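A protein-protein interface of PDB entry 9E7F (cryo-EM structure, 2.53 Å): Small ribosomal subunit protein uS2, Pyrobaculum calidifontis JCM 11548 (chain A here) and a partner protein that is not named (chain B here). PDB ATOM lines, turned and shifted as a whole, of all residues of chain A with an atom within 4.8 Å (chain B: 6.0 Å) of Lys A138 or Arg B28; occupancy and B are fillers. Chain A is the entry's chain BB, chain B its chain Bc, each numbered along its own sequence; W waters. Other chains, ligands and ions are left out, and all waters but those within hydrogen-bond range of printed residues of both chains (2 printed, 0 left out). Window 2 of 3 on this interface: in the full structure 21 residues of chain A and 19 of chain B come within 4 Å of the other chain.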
ATOM      1  N   ALA A 134       2.458  -0.901 -20.263  1.00  0.00           N
ATOM      2  CA  ALA A 134       2.628   0.548 -20.276  1.00  0.00           C
ATOM      3  C   ALA A 134       2.255   1.141 -21.625  1.00  0.00           C
ATOM      4  O   ALA A 134       1.608   2.191 -21.692  1.00  0.00           O
ATOM      5  CB  ALA A 134       4.066   0.909 -19.919  1.00  0.00           C
ATOM      6  N   GLU A 135       2.657   0.490 -22.713  1.00  0.00           N
ATOM      7  CA  GLU A 135       2.294   0.994 -24.029  1.00  0.00           C
ATOM      8  C   GLU A 135       0.812   0.801 -24.307  1.00  0.00           C
ATOM      9  O   GLU A 135       0.217   1.576 -25.062  1.00  0.00           O
ATOM     10  CB  GLU A 135       3.144   0.315 -25.098  1.00  0.00           C
ATOM     11  CG  GLU A 135       4.629   0.549 -24.921  1.00  0.00           C
ATOM     12  CD  GLU A 135       5.373   0.640 -26.239  1.00  0.00           C
ATOM     13  OE1 GLU A 135       5.236  -0.279 -27.065  1.00  0.00           O
ATOM     14  OE2 GLU A 135       6.097   1.633 -26.450  1.00  0.00           O
ATOM     15  N   ALA A 136       0.204  -0.224 -23.709  1.00  0.00           N
ATOM     16  CA  ALA A 136      -1.230  -0.434 -23.872  1.00  0.00           C
ATOM     17  C   ALA A 136      -2.029   0.691 -23.235  1.00  0.00           C
ATOM     18  O   ALA A 136      -3.026   1.153 -23.803  1.00  0.00           O
ATOM     19  CB  ALA A 136      -1.634  -1.776 -23.268  1.00  0.00           C
ATOM     20  N   ALA A 137      -1.624   1.130 -22.044  1.00  0.00           N
ATOM     21  CA  ALA A 137      -2.313   2.232 -21.385  1.00  0.00           C
ATOM     22  C   ALA A 137      -2.181   3.517 -22.185  1.00  0.00           C
ATOM     23  O   ALA A 137      -3.150   4.269 -22.335  1.00  0.00           O
ATOM     24  CB  ALA A 137      -1.761   2.420 -19.974  1.00  0.00           C
ATOM     25  N   LYS A 138      -0.988   3.786 -22.705  1.00  0.00           N
ATOM     26  CA  LYS A 138      -0.780   4.993 -23.491  1.00  0.00           C
ATOM     27  C   LYS A 138      -1.504   4.915 -24.827  1.00  0.00           C
ATOM     28  O   LYS A 138      -2.044   5.916 -25.307  1.00  0.00           O
ATOM     29  CB  LYS A 138       0.715   5.220 -23.700  1.00  0.00           C
ATOM     30  CG  LYS A 138       1.044   6.385 -24.602  1.00  0.00           C
ATOM     31  CD  LYS A 138       1.451   7.608 -23.803  1.00  0.00           C
ATOM     32  CE  LYS A 138       2.557   8.376 -24.494  1.00  0.00           C
ATOM     33  NZ  LYS A 138       3.349   9.190 -23.541  1.00  0.00           N
ATOM     34  N   MET A 139      -1.526   3.735 -25.441  1.00  0.00           N
ATOM     35  CA  MET A 139      -2.069   3.561 -26.779  1.00  0.00           C
ATOM     36  C   MET A 139      -3.525   3.127 -26.776  1.00  0.00           C
ATOM     37  O   MET A 139      -4.104   2.957 -27.851  1.00  0.00           O
ATOM     38  CB  MET A 139      -1.235   2.543 -27.551  1.00  0.00           C
ATOM     39  CG  MET A 139      -1.031   2.881 -29.009  1.00  0.00           C
ATOM     40  SD  MET A 139       0.241   4.133 -29.222  1.00  0.00           S
ATOM     41  CE  MET A 139      -0.746   5.536 -29.693  1.00  0.00           C
ATOM     42  N   GLY A 140      -4.122   2.933 -25.607  1.00  0.00           N
ATOM     43  CA  GLY A 140      -5.530   2.609 -25.514  1.00  0.00           C
ATOM     44  C   GLY A 140      -5.923   1.288 -26.137  1.00  0.00           C
ATOM     45  O   GLY A 140      -6.891   1.217 -26.898  1.00  0.00           O
ATOM     46  N   LEU B  23     -13.936  10.453 -22.072  1.00  0.00           N
ATOM     47  CA  LEU B  23     -12.686  10.034 -22.680  1.00  0.00           C
ATOM     48  C   LEU B  23     -12.140  11.231 -23.436  1.00  0.00           C
ATOM     49  O   LEU B  23     -12.478  11.455 -24.602  1.00  0.00           O
ATOM     50  CB  LEU B  23     -12.882   8.834 -23.603  1.00  0.00           C
ATOM     51  CG  LEU B  23     -12.843   7.444 -22.973  1.00  0.00           C
ATOM     52  CD1 LEU B  23     -13.763   7.341 -21.778  1.00  0.00           C
ATOM     53  CD2 LEU B  23     -13.194   6.389 -23.991  1.00  0.00           C
ATOM     54  N   ALA B  24     -11.301  12.009 -22.764  1.00  0.00           N
ATOM     55  CA  ALA B  24     -10.881  13.287 -23.287  1.00  0.00           C
ATOM     56  C   ALA B  24      -9.968  13.102 -24.492  1.00  0.00           C
ATOM     57  O   ALA B  24      -9.386  12.034 -24.686  1.00  0.00           O
ATOM     58  CB  ALA B  24     -10.171  14.088 -22.201  1.00  0.00           C
ATOM     59  N   LEU B  26      -6.642  13.170 -26.509  1.00  0.00           N
ATOM     60  CA  LEU B  26      -5.236  12.908 -26.202  1.00  0.00           C
ATOM     61  C   LEU B  26      -5.037  12.008 -24.987  1.00  0.00           C
ATOM     62  O   LEU B  26      -3.904  11.620 -24.693  1.00  0.00           O
ATOM     63  CB  LEU B  26      -4.462  14.214 -26.008  1.00  0.00           C
ATOM     64  CG  LEU B  26      -4.586  15.265 -27.108  1.00  0.00           C
ATOM     65  CD1 LEU B  26      -4.466  16.657 -26.525  1.00  0.00           C
ATOM     66  CD2 LEU B  26      -3.527  15.038 -28.165  1.00  0.00           C
ATOM     67  N   GLU B  27      -6.110  11.663 -24.282  1.00  0.00           N
ATOM     68  CA  GLU B  27      -6.035  10.665 -23.222  1.00  0.00           C
ATOM     69  C   GLU B  27      -6.893   9.472 -23.605  1.00  0.00           C
ATOM     70  O   GLU B  27      -8.124   9.557 -23.598  1.00  0.00           O
ATOM     71  CB  GLU B  27      -6.500  11.259 -21.894  1.00  0.00           C
ATOM     72  CG  GLU B  27      -6.493  10.270 -20.741  1.00  0.00           C
ATOM     73  CD  GLU B  27      -6.643  10.938 -19.386  1.00  0.00           C
ATOM     74  OE1 GLU B  27      -6.337  12.142 -19.281  1.00  0.00           O
ATOM     75  OE2 GLU B  27      -7.067  10.259 -18.425  1.00  0.00           O
ATOM     76  N   ARG B  28      -6.255   8.359 -23.933  1.00  0.00           N
ATOM     77  CA  ARG B  28      -6.916   7.305 -24.683  1.00  0.00           C
ATOM     78  C   ARG B  28      -7.624   6.354 -23.733  1.00  0.00           C
ATOM     79  O   ARG B  28      -6.983   5.707 -22.901  1.00  0.00           O
ATOM     80  CB  ARG B  28      -5.920   6.542 -25.551  1.00  0.00           C
ATOM     81  CG  ARG B  28      -6.189   6.693 -27.033  1.00  0.00           C
ATOM     82  CD  ARG B  28      -5.823   5.442 -27.775  1.00  0.00           C
ATOM     83  NE  ARG B  28      -6.880   4.445 -27.669  1.00  0.00           N
ATOM     84  CZ  ARG B  28      -7.960   4.417 -28.437  1.00  0.00           C
ATOM     85  NH1 ARG B  28      -8.137   5.290 -29.413  1.00  0.00           N
ATOM     86  NH2 ARG B  28      -8.883   3.484 -28.224  1.00  0.00           N
ATOM     87  N   GLY B  29      -8.942   6.266 -23.869  1.00  0.00           N
ATOM     88  CA  GLY B  29      -9.720   5.254 -23.196  1.00  0.00           C
ATOM     89  C   GLY B  29      -9.672   3.945 -23.951  1.00  0.00           C
ATOM     90  O   GLY B  29      -8.798   3.703 -24.784  1.00  0.00           O
ATOM     91  N   VAL B  30     -10.638   3.086 -23.656  1.00  0.00           N
ATOM     92  CA  VAL B  30     -10.706   1.767 -24.265  1.00  0.00           C
ATOM     93  C   VAL B  30     -12.162   1.343 -24.368  1.00  0.00           C
ATOM     94  O   VAL B  30     -12.925   1.465 -23.406  1.00  0.00           O
ATOM     95  CB  VAL B  30      -9.884   0.740 -23.467  1.00  0.00           C
ATOM     96  CG1 VAL B  30     -10.370  -0.646 -23.751  1.00  0.00           C
ATOM     97  CG2 VAL B  30      -8.425   0.854 -23.830  1.00  0.00           C
ATOM     98  N   VAL B  31     -12.543   0.838 -25.538  1.00  0.00           N
ATOM     99  CA  VAL B  31     -13.912   0.432 -25.821  1.00  0.00           C
ATOM    100  C   VAL B  31     -13.905  -1.009 -26.303  1.00  0.00           C
ATOM    101  O   VAL B  31     -13.063  -1.389 -27.122  1.00  0.00           O
ATOM    102  CB  VAL B  31     -14.575   1.338 -26.874  1.00  0.00           C
ATOM    103  CG1 VAL B  31     -16.079   1.270 -26.741  1.00  0.00           C
ATOM    104  CG2 VAL B  31     -14.080   2.765 -26.740  1.00  0.00           C
ATOM    105  N   ARG B  44     -14.144   2.485 -20.952  1.00  0.00           N
ATOM    106  CA  ARG B  44     -13.305   2.687 -19.776  1.00  0.00           C
ATOM    107  C   ARG B  44     -12.357   3.843 -20.049  1.00  0.00           C
ATOM    108  O   ARG B  44     -11.464   3.729 -20.892  1.00  0.00           O
ATOM    109  CB  ARG B  44     -12.528   1.419 -19.433  1.00  0.00           C
ATOM    110  CG  ARG B  44     -13.075   0.669 -18.248  1.00  0.00           C
ATOM    111  CD  ARG B  44     -12.625  -0.774 -18.246  1.00  0.00           C
ATOM    112  NE  ARG B  44     -11.376  -0.983 -17.523  1.00  0.00           N
ATOM    113  CZ  ARG B  44     -11.246  -0.906 -16.206  1.00  0.00           C
ATOM    114  NH1 ARG B  44     -12.262  -0.584 -15.426  1.00  0.00           N
ATOM    115  NH2 ARG B  44     -10.065  -1.166 -15.656  1.00  0.00           N
ATOM    116  N   SER B  45     -12.540   4.946 -19.333  1.00  0.00           N
ATOM    117  CA  SER B  45     -11.620   6.062 -19.451  1.00  0.00           C
ATOM    118  C   SER B  45     -10.253   5.677 -18.895  1.00  0.00           C
ATOM    119  O   SER B  45     -10.094   4.662 -18.213  1.00  0.00           O
ATOM    120  CB  SER B  45     -12.162   7.285 -18.715  1.00  0.00           C
ATOM    121  OG  SER B  45     -11.137   8.228 -18.480  1.00  0.00           O
ATOM    122  N   ALA B  46      -9.251   6.499 -19.209  1.00  0.00           N
ATOM    123  CA  ALA B  46      -7.894   6.209 -18.761  1.00  0.00           C
ATOM    124  C   ALA B  46      -7.778   6.268 -17.248  1.00  0.00           C
ATOM    125  O   ALA B  46      -6.964   5.549 -16.660  1.00  0.00           O
ATOM    126  CB  ALA B  46      -6.912   7.182 -19.405  1.00  0.00           C
ATOM    127  N   ARG B  49      -9.119   2.875 -15.825  1.00  0.00           N
ATOM    128  CA  ARG B  49      -8.193   1.774 -16.061  1.00  0.00           C
ATOM    129  C   ARG B  49      -7.048   1.794 -15.064  1.00  0.00           C
ATOM    130  O   ARG B  49      -6.620   0.742 -14.581  1.00  0.00           O
ATOM    131  CB  ARG B  49      -7.659   1.828 -17.491  1.00  0.00           C
ATOM    132  CG  ARG B  49      -8.740   1.969 -18.537  1.00  0.00           C
ATOM    133  CD  ARG B  49      -8.191   2.415 -19.873  1.00  0.00           C
ATOM    134  NE  ARG B  49      -6.887   1.844 -20.179  1.00  0.00           N
ATOM    135  CZ  ARG B  49      -6.706   0.634 -20.686  1.00  0.00           C
ATOM    136  NH1 ARG B  49      -7.721  -0.175 -20.909  1.00  0.00           N
ATOM    137  NH2 ARG B  49      -5.477   0.232 -20.985  1.00  0.00           N
HETATM  138  O   HOH W   1      -5.473   4.447 -20.714  1.00  0.00           O
HETATM  139  O   HOH W   2      -3.221   8.103 -23.491  1.00  0.00           O
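The guanidinium group (NE) of Arg B28 sits close to the backbone carbonyl oxygen (O) of Met A139, at 3.2 Å. O of Gly A140 sits at hydrogen-bond distance from NH2 of Arg B28 (3.3 Å).
The backbone carbonyl oxygen (O) of Val B30 lies within hydrogen-bond range of the backbone NH (N) of Arg B44, at 2.9 Å.
Arg B49 touches Ala A136 (NH2 to O, 3.8 Å). NH2 of Arg B49 touches CA of Ala A137 (3.8 Å). O of Lys A138 touches CB of Arg B28, 3.9 Å away. CA of Gly A140 touches O of Gly B29, 3.5 Å away. Val B30 touches Gly A140 (CG2 to C, 3.4 Å).
Ala A134 touches none of the printed residues of chain B. Printed residues of chain B within 4 Å of Ala A136: Arg B49 (3.8 Å). Of chain B, only Arg B28 (3.9 Å) comes within 4 Å of Lys A138. Printed residues of chain B within 4 Å of Met A139: Arg B28 (3.0 Å). Of the printed residues of chain B, Gly A140 touches Arg B28 (3.1 Å), Gly B29 (3.5 Å) and Val B30 (3.4 Å). Arg B28 touches three residues of chain A. Of the printed residues of chain A, Gly B29 touches Gly A140. The nearest printed residue of chain B that does not touch Gly A140 is Arg B49 (5.1 Å).
Of the 12 printed residues of chain B, 4 touch a printed residue of chain A. Hydrophobic or aromatic side chains of chain B that line the printed part of chain A: Val B30. Along chain B the printed residues that touch a printed residue of chain A span positions 28 to 49. Among the printed residues, 7 pairs touch across the chains. Among the printed residues, no Asp or Glu carboxylate lies within 4 Å of a Lys or Arg side-chain nitrogen of the other chain.
Water W1 lies within hydrogen-bond range of the backbone carbonyl oxygen (O) of Ala A137 (2.8 Å), the backbone carbonyl oxygen (O) of Arg B28 (2.9 Å) and the guanidinium group (NE) of Arg B49 (3.0 Å). Water W2 bridges N of Arg B28 (3.1 Å) and O of Lys A138 (3.1 Å).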
